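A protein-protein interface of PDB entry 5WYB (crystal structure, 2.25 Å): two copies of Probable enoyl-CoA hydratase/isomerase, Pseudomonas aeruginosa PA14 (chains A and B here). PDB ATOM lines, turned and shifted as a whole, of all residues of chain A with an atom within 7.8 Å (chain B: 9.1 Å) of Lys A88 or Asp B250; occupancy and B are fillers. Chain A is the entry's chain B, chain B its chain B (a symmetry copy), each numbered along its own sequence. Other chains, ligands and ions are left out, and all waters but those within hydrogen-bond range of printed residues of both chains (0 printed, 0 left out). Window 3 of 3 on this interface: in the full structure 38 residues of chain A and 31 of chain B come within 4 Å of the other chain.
Among the printed residues, pairs that only touch across the chains: Ala A84 with Phe B249 (3.999 Å), Gly A86 with Phe B249 (3.6 Å), Asp A87 with Phe B249 (3.5 Å), Lys A88 with Asp B250 (3.1 Å), Ala A91 with Phe B249 (3.5 Å), Arg A92 with Val B246 (3.9 Å), Gly A150 with Ser B215 (3.5 Å), Gly A150 with Leu B248 (3.5 Å), Leu A151 with Phe B245 (3.9 Å) and Leu A151 with Leu B248 (3.7 Å).
Asp A85 touches none of the printed residues of chain B.
Of chain B, only Asp B250 comes within 4 Å of Lys A88.
Of the printed residues of chain B, Arg A92 touches Val B246.
Val B217 touches none of the printed residues of chain A.
Of the printed residues of chain A, Phe B249 touches Ala A84, Gly A86, Asp A87 and Ala A91.
Of the printed residues of chain A, Asp B250 touches Lys A88 (3.1 Å).
The nearest residue of chain B that does not touch Lys A88 is Phe B249 (4.2 Å).
The nearest residue of chain A that does not touch Asp B250 is Leu A151 (6.4 Å).
The nearest printed residue of chain B that does not touch Leu A151 is Phe B249 (4.02 Å).
Of the 13 printed residues of chain B, 6 touch a printed residue of chain A.
Hydrophobic or aromatic side chains of chain B within 4 Å of the printed part of chain A: Phe B245, Val B246, Leu B248 and Phe B249.
Of the 13 printed residues of chain A, 8 touch a printed residue of chain B.
Printed residues of chain A that touch a printed residue of chain B: Ala A84, Gly A86, Asp A87, Lys A88, Ala A91, Arg A92, Gly A150 and Leu A151.
Hydrophobic or aromatic side chains of chain A that line the printed part of chain B: Ala A91 and Leu A151.
Among the printed residues, no Asp or Glu carboxylate lies within 4 Å of a Lys or Arg side-chain nitrogen of the other chain.
No position is printed for both chains.
Of the 10 pairs that touch across the chains among the printed residues, none has its exchanged pair printed and touching as well.
The side-chain carboxylate (OD1) of Asp A87 lies within hydrogen-bond range of the backbone NH (N) of Ala A89 (2.9 Å).
The side-chain carboxylate (OE1) of Glu A93 lies within salt-bridge range of the guanidinium group (NH1) of Arg A92, at 3.4 Å.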
ATOM      1  N   ALA A  84      -9.317 -16.860  -4.143  1.00  0.00           N
ATOM      2  CA  ALA A  84      -8.115 -16.208  -4.630  1.00  0.00           C
ATOM      3  C   ALA A  84      -7.086 -15.926  -3.525  1.00  0.00           C
ATOM      4  O   ALA A  84      -7.426 -15.599  -2.400  1.00  0.00           O
ATOM      5  CB  ALA A  84      -8.505 -14.899  -5.312  1.00  0.00           C
ATOM      6  N   ASP A  85      -5.819 -16.039  -3.852  1.00  0.00           N
ATOM      7  CA  ASP A  85      -4.816 -15.732  -2.860  1.00  0.00           C
ATOM      8  C   ASP A  85      -5.099 -16.561  -1.580  1.00  0.00           C
ATOM      9  O   ASP A  85      -5.139 -17.772  -1.721  1.00  0.00           O
ATOM     10  CB  ASP A  85      -4.610 -14.222  -2.724  1.00  0.00           C
ATOM     11  CG  ASP A  85      -4.046 -13.600  -3.982  1.00  0.00           C
ATOM     12  OD1 ASP A  85      -3.139 -14.205  -4.578  1.00  0.00           O
ATOM     13  OD2 ASP A  85      -4.508 -12.505  -4.370  1.00  0.00           O
ATOM     14  N   GLY A  86      -5.228 -15.982  -0.382  1.00  0.00           N
ATOM     15  CA  GLY A  86      -5.247 -14.557  -0.129  1.00  0.00           C
ATOM     16  C   GLY A  86      -6.376 -14.015   0.749  1.00  0.00           C
ATOM     17  O   GLY A  86      -6.426 -14.323   1.928  1.00  0.00           O
ATOM     18  N   ASP A  87      -7.279 -13.215   0.207  1.00  0.00           N
ATOM     19  CA  ASP A  87      -8.292 -12.575   1.040  1.00  0.00           C
ATOM     20  C   ASP A  87      -9.106 -13.550   1.856  1.00  0.00           C
ATOM     21  O   ASP A  87      -9.800 -14.391   1.334  1.00  0.00           O
ATOM     22  CB  ASP A  87      -9.216 -11.764   0.108  1.00  0.00           C
ATOM     23  CG  ASP A  87      -9.992 -10.652   0.808  1.00  0.00           C
ATOM     24  OD1 ASP A  87     -10.145 -10.663   2.032  1.00  0.00           O
ATOM     25  OD2 ASP A  87     -10.469  -9.740   0.113  1.00  0.00           O
ATOM     26  N   LYS A  88      -9.033 -13.377   3.165  1.00  0.00           N
ATOM     27  CA  LYS A  88      -9.785 -14.145   4.141  1.00  0.00           C
ATOM     28  C   LYS A  88     -11.238 -13.814   4.020  1.00  0.00           C
ATOM     29  O   LYS A  88     -12.088 -14.627   4.247  1.00  0.00           O
ATOM     30  CB  LYS A  88      -9.327 -13.850   5.545  1.00  0.00           C
ATOM     31  CG  LYS A  88      -7.854 -13.940   5.731  1.00  0.00           C
ATOM     32  CD  LYS A  88      -7.563 -14.229   7.158  1.00  0.00           C
ATOM     33  CE  LYS A  88      -6.075 -14.189   7.401  1.00  0.00           C
ATOM     34  NZ  LYS A  88      -5.743 -14.159   8.836  1.00  0.00           N
ATOM     35  N   ALA A  89     -11.494 -12.559   3.705  1.00  0.00           N
ATOM     36  CA  ALA A  89     -12.860 -12.074   3.549  1.00  0.00           C
ATOM     37  C   ALA A  89     -13.531 -12.692   2.331  1.00  0.00           C
ATOM     38  O   ALA A  89     -14.712 -13.054   2.388  1.00  0.00           O
ATOM     39  CB  ALA A  89     -12.867 -10.551   3.452  1.00  0.00           C
ATOM     40  N   ARG A  90     -12.795 -12.825   1.221  1.00  0.00           N
ATOM     41  CA  ARG A  90     -13.346 -13.480   0.037  1.00  0.00           C
ATOM     42  C   ARG A  90     -13.797 -14.893   0.348  1.00  0.00           C
ATOM     43  O   ARG A  90     -14.890 -15.306  -0.049  1.00  0.00           O
ATOM     44  CB  ARG A  90     -12.315 -13.528  -1.085  1.00  0.00           C
ATOM     45  CG  ARG A  90     -12.135 -12.238  -1.825  1.00  0.00           C
ATOM     46  CD  ARG A  90     -13.366 -11.813  -2.609  1.00  0.00           C
ATOM     47  NE  ARG A  90     -13.978 -12.806  -3.491  1.00  0.00           N
ATOM     48  CZ  ARG A  90     -13.358 -13.526  -4.419  1.00  0.00           C
ATOM     49  NH1 ARG A  90     -14.088 -14.340  -5.172  1.00  0.00           N
ATOM     50  NH2 ARG A  90     -12.038 -13.456  -4.585  1.00  0.00           N
ATOM     51  N   ALA A  91     -12.955 -15.655   1.046  1.00  0.00           N
ATOM     52  CA  ALA A  91     -13.243 -17.064   1.271  1.00  0.00           C
ATOM     53  C   ALA A  91     -14.560 -17.240   2.006  1.00  0.00           C
ATOM     54  O   ALA A  91     -15.376 -18.096   1.648  1.00  0.00           O
ATOM     55  CB  ALA A  91     -12.103 -17.712   2.051  1.00  0.00           C
ATOM     56  N   ARG A  92     -14.771 -16.442   3.031  1.00  0.00           N
ATOM     57  CA  ARG A  92     -15.971 -16.532   3.815  1.00  0.00           C
ATOM     58  C   ARG A  92     -17.220 -16.221   3.025  1.00  0.00           C
ATOM     59  O   ARG A  92     -18.180 -16.914   3.114  1.00  0.00           O
ATOM     60  CB  ARG A  92     -15.806 -15.601   5.004  1.00  0.00           C
ATOM     61  CG  ARG A  92     -16.780 -15.796   6.116  1.00  0.00           C
ATOM     62  CD  ARG A  92     -17.912 -14.849   5.953  1.00  0.00           C
ATOM     63  NE  ARG A  92     -18.967 -15.203   6.852  1.00  0.00           N
ATOM     64  CZ  ARG A  92     -20.204 -14.849   6.662  1.00  0.00           C
ATOM     65  NH1 ARG A  92     -20.520 -14.121   5.638  1.00  0.00           N
ATOM     66  NH2 ARG A  92     -21.108 -15.240   7.497  1.00  0.00           N
ATOM     67  N   GLU A  93     -17.183 -15.187   2.224  1.00  0.00           N
ATOM     68  CA  GLU A  93     -18.306 -14.824   1.405  1.00  0.00           C
ATOM     69  C   GLU A  93     -18.600 -15.896   0.390  1.00  0.00           C
ATOM     70  O   GLU A  93     -19.718 -16.119   0.013  1.00  0.00           O
ATOM     71  CB  GLU A  93     -18.109 -13.507   0.701  1.00  0.00           C
ATOM     72  CG  GLU A  93     -19.405 -12.743   0.506  1.00  0.00           C
ATOM     73  CD  GLU A  93     -20.150 -12.405   1.812  1.00  0.00           C
ATOM     74  OE1 GLU A  93     -19.518 -12.297   2.889  1.00  0.00           O
ATOM     75  OE2 GLU A  93     -21.384 -12.235   1.771  1.00  0.00           O
ATOM     76  N   MET A  94     -17.550 -16.521  -0.090  1.00  0.00           N
ATOM     77  CA  MET A  94     -17.715 -17.559  -1.091  1.00  0.00           C
ATOM     78  C   MET A  94     -18.325 -18.816  -0.495  1.00  0.00           C
ATOM     79  O   MET A  94     -19.213 -19.424  -1.104  1.00  0.00           O
ATOM     80  CB  MET A  94     -16.378 -17.854  -1.743  1.00  0.00           C
ATOM     81  CG  MET A  94     -16.278 -17.265  -3.112  1.00  0.00           C
ATOM     82  SD  MET A  94     -16.654 -15.507  -3.228  1.00  0.00           S
ATOM     83  CE  MET A  94     -18.245 -15.551  -4.040  1.00  0.00           C
ATOM     84  N   GLY A 150      -5.645 -28.623   1.259  1.00  0.00           N
ATOM     85  CA  GLY A 150      -5.837 -28.144   2.610  1.00  0.00           C
ATOM     86  C   GLY A 150      -7.161 -27.469   2.873  1.00  0.00           C
ATOM     87  O   GLY A 150      -7.253 -26.659   3.795  1.00  0.00           O
ATOM     88  N   LEU A 151      -8.187 -27.769   2.082  1.00  0.00           N
ATOM     89  CA  LEU A 151      -9.500 -27.174   2.274  1.00  0.00           C
ATOM     90  C   LEU A 151     -10.522 -28.273   2.511  1.00  0.00           C
ATOM     91  O   LEU A 151     -10.154 -29.371   2.931  1.00  0.00           O
ATOM     92  CB  LEU A 151      -9.872 -26.302   1.077  1.00  0.00           C
ATOM     93  CG  LEU A 151      -8.928 -25.112   0.873  1.00  0.00           C
ATOM     94  CD1 LEU A 151      -9.380 -24.223  -0.256  1.00  0.00           C
ATOM     95  CD2 LEU A 151      -8.801 -24.302   2.157  1.00  0.00           C
ATOM     96  N   SER B 215      -3.472 -32.780   3.082  1.00  0.00           N
ATOM     97  CA  SER B 215      -3.172 -31.962   4.246  1.00  0.00           C
ATOM     98  C   SER B 215      -3.635 -32.671   5.512  1.00  0.00           C
ATOM     99  O   SER B 215      -4.828 -32.984   5.634  1.00  0.00           O
ATOM    100  CB  SER B 215      -3.845 -30.602   4.123  1.00  0.00           C
ATOM    101  OG  SER B 215      -3.709 -29.847   5.313  1.00  0.00           O
ATOM    102  N   VAL B 217      -3.928 -31.425   8.544  1.00  0.00           N
ATOM    103  CA  VAL B 217      -4.831 -30.565   9.302  1.00  0.00           C
ATOM    104  C   VAL B 217      -6.206 -30.539   8.653  1.00  0.00           C
ATOM    105  O   VAL B 217      -7.217 -30.324   9.331  1.00  0.00           O
ATOM    106  CB  VAL B 217      -4.231 -29.151   9.456  1.00  0.00           C
ATOM    107  CG1 VAL B 217      -4.320 -28.380   8.159  1.00  0.00           C
ATOM    108  CG2 VAL B 217      -4.929 -28.400  10.576  1.00  0.00           C
ATOM    109  N   ARG B 242     -18.930 -24.458   6.907  1.00  0.00           N
ATOM    110  CA  ARG B 242     -18.313 -23.242   6.380  1.00  0.00           C
ATOM    111  C   ARG B 242     -17.325 -22.639   7.370  1.00  0.00           C
ATOM    112  O   ARG B 242     -16.273 -22.123   6.973  1.00  0.00           O
ATOM    113  CB  ARG B 242     -19.387 -22.215   6.040  1.00  0.00           C
ATOM    114  CG  ARG B 242     -20.497 -22.761   5.203  1.00  0.00           C
ATOM    115  CD  ARG B 242     -21.601 -21.744   5.015  1.00  0.00           C
ATOM    116  NE  ARG B 242     -22.816 -22.429   4.612  1.00  0.00           N
ATOM    117  CZ  ARG B 242     -23.895 -22.548   5.370  1.00  0.00           C
ATOM    118  NH1 ARG B 242     -23.928 -21.997   6.569  1.00  0.00           N
ATOM    119  NH2 ARG B 242     -24.947 -23.213   4.918  1.00  0.00           N
ATOM    120  N   GLU B 243     -17.655 -22.676   8.658  1.00  0.00           N
ATOM    121  CA  GLU B 243     -16.785 -22.075   9.661  1.00  0.00           C
ATOM    122  C   GLU B 243     -15.433 -22.771   9.698  1.00  0.00           C
ATOM    123  O   GLU B 243     -14.383 -22.120   9.673  1.00  0.00           O
ATOM    124  CB  GLU B 243     -17.472 -22.119  11.028  1.00  0.00           C
ATOM    125  CG  GLU B 243     -16.552 -21.947  12.210  1.00  0.00           C
ATOM    126  CD  GLU B 243     -17.318 -21.966  13.522  1.00  0.00           C
ATOM    127  OE1 GLU B 243     -18.126 -21.045  13.741  1.00  0.00           O
ATOM    128  OE2 GLU B 243     -17.133 -22.906  14.319  1.00  0.00           O
ATOM    129  N   ARG B 244     -15.438 -24.103   9.736  1.00  0.00           N
ATOM    130  CA  ARG B 244     -14.182 -24.837   9.667  1.00  0.00           C
ATOM    131  C   ARG B 244     -13.531 -24.730   8.295  1.00  0.00           C
ATOM    132  O   ARG B 244     -12.312 -24.888   8.187  1.00  0.00           O
ATOM    133  CB  ARG B 244     -14.416 -26.296  10.046  1.00  0.00           C
ATOM    134  CG  ARG B 244     -14.849 -26.458  11.490  1.00  0.00           C
ATOM    135  CD  ARG B 244     -15.320 -27.864  11.800  1.00  0.00           C
ATOM    136  NE  ARG B 244     -14.239 -28.746  12.229  1.00  0.00           N
ATOM    137  CZ  ARG B 244     -14.405 -29.769  13.062  1.00  0.00           C
ATOM    138  NH1 ARG B 244     -15.607 -30.026  13.565  1.00  0.00           N
ATOM    139  NH2 ARG B 244     -13.373 -30.526  13.405  1.00  0.00           N
ATOM    140  N   PHE B 245     -14.303 -24.449   7.249  1.00  0.00           N
ATOM    141  CA  PHE B 245     -13.688 -24.176   5.956  1.00  0.00           C
ATOM    142  C   PHE B 245     -12.854 -22.901   6.001  1.00  0.00           C
ATOM    143  O   PHE B 245     -11.749 -22.858   5.448  1.00  0.00           O
ATOM    144  CB  PHE B 245     -14.750 -24.071   4.872  1.00  0.00           C
ATOM    145  CG  PHE B 245     -14.214 -23.577   3.568  1.00  0.00           C
ATOM    146  CD1 PHE B 245     -13.535 -24.430   2.715  1.00  0.00           C
ATOM    147  CD2 PHE B 245     -14.376 -22.262   3.198  1.00  0.00           C
ATOM    148  CE1 PHE B 245     -13.032 -23.975   1.516  1.00  0.00           C
ATOM    149  CE2 PHE B 245     -13.874 -21.797   2.011  1.00  0.00           C
ATOM    150  CZ  PHE B 245     -13.201 -22.654   1.168  1.00  0.00           C
ATOM    151  N   VAL B 246     -13.368 -21.846   6.648  1.00  0.00           N
ATOM    152  CA  VAL B 246     -12.598 -20.613   6.773  1.00  0.00           C
ATOM    153  C   VAL B 246     -11.420 -20.819   7.712  1.00  0.00           C
ATOM    154  O   VAL B 246     -10.327 -20.288   7.483  1.00  0.00           O
ATOM    155  CB  VAL B 246     -13.501 -19.456   7.231  1.00  0.00           C
ATOM    156  CG1 VAL B 246     -12.702 -18.171   7.336  1.00  0.00           C
ATOM    157  CG2 VAL B 246     -14.661 -19.281   6.271  1.00  0.00           C
ATOM    158  N   ASP B 247     -11.610 -21.607   8.771  1.00  0.00           N
ATOM    159  CA  ASP B 247     -10.490 -21.946   9.640  1.00  0.00           C
ATOM    160  C   ASP B 247      -9.384 -22.635   8.857  1.00  0.00           C
ATOM    161  O   ASP B 247      -8.198 -22.410   9.119  1.00  0.00           O
ATOM    162  CB  ASP B 247     -10.954 -22.838  10.790  1.00  0.00           C
ATOM    163  CG  ASP B 247     -12.043 -22.200  11.624  1.00  0.00           C
ATOM    164  OD1 ASP B 247     -12.118 -20.954  11.668  1.00  0.00           O
ATOM    165  OD2 ASP B 247     -12.825 -22.952  12.243  1.00  0.00           O
ATOM    166  N   LEU B 248      -9.752 -23.480   7.890  1.00  0.00           N
ATOM    167  CA  LEU B 248      -8.746 -24.095   7.034  1.00  0.00           C
ATOM    168  C   LEU B 248      -8.175 -23.107   6.030  1.00  0.00           C
ATOM    169  O   LEU B 248      -6.994 -23.202   5.683  1.00  0.00           O
ATOM    170  CB  LEU B 248      -9.332 -25.306   6.307  1.00  0.00           C
ATOM    171  CG  LEU B 248      -9.544 -26.575   7.137  1.00  0.00           C
ATOM    172  CD1 LEU B 248     -10.088 -27.681   6.264  1.00  0.00           C
ATOM    173  CD2 LEU B 248      -8.253 -27.014   7.821  1.00  0.00           C
ATOM    174  N   PHE B 249      -8.981 -22.160   5.550  1.00  0.00           N
ATOM    175  CA  PHE B 249      -8.445 -21.150   4.647  1.00  0.00           C
ATOM    176  C   PHE B 249      -7.423 -20.270   5.356  1.00  0.00           C
ATOM    177  O   PHE B 249      -6.387 -19.923   4.778  1.00  0.00           O
ATOM    178  CB  PHE B 249      -9.568 -20.305   4.061  1.00  0.00           C
ATOM    179  CG  PHE B 249      -9.136 -19.454   2.902  1.00  0.00           C
ATOM    180  CD1 PHE B 249      -8.632 -18.179   3.105  1.00  0.00           C
ATOM    181  CD2 PHE B 249      -9.226 -19.935   1.607  1.00  0.00           C
ATOM    182  CE1 PHE B 249      -8.233 -17.400   2.037  1.00  0.00           C
ATOM    183  CE2 PHE B 249      -8.828 -19.163   0.533  1.00  0.00           C
ATOM    184  CZ  PHE B 249      -8.331 -17.893   0.748  1.00  0.00           C
ATOM    185  N   ASP B 250      -7.701 -19.886   6.598  1.00  0.00           N
ATOM    186  CA  ASP B 250      -6.654 -19.314   7.428  1.00  0.00           C
ATOM    187  C   ASP B 250      -5.555 -20.352   7.615  1.00  0.00           C
ATOM    188  O   ASP B 250      -5.799 -21.559   7.547  1.00  0.00           O
ATOM    189  CB  ASP B 250      -7.214 -18.878   8.783  1.00  0.00           C
ATOM    190  CG  ASP B 250      -8.471 -18.037   8.652  1.00  0.00           C
ATOM    191  OD1 ASP B 250      -8.511 -17.136   7.792  1.00  0.00           O
ATOM    192  OD2 ASP B 250      -9.430 -18.287   9.408  1.00  0.00           O
ATOM    193  N   ALA B 251      -4.335 -19.872   7.845  1.00  0.00           N
ATOM    194  CA  ALA B 251      -3.148 -20.727   7.836  1.00  0.00           C
ATOM    195  C   ALA B 251      -3.018 -21.454   6.499  1.00  0.00           C
ATOM    196  O   ALA B 251      -2.710 -22.646   6.446  1.00  0.00           O
ATOM    197  CB  ALA B 251      -3.156 -21.720   9.002  1.00  0.00           C
ATOM    198  N   GLN B 252      -3.225 -20.684   5.441  1.00  0.00           N
ATOM    199  CA  GLN B 252      -3.138 -21.165   4.090  1.00  0.00           C
ATOM    200  C   GLN B 252      -3.886 -22.447   3.862  1.00  0.00           C
ATOM    201  O   GLN B 252      -4.663 -22.537   2.936  1.00  0.00           O
ATOM    202  CB  GLN B 252      -1.691 -21.240   3.619  1.00  0.00           C
ATOM    203  CG  GLN B 252      -0.633 -21.247   4.705  1.00  0.00           C
ATOM    204  CD  GLN B 252      -0.093 -19.875   5.065  1.00  0.00           C
ATOM    205  OE1 GLN B 252       1.001 -19.748   5.649  1.00  0.00           O
ATOM    206  NE2 GLN B 252      -0.857 -18.832   4.729  1.00  0.00           N
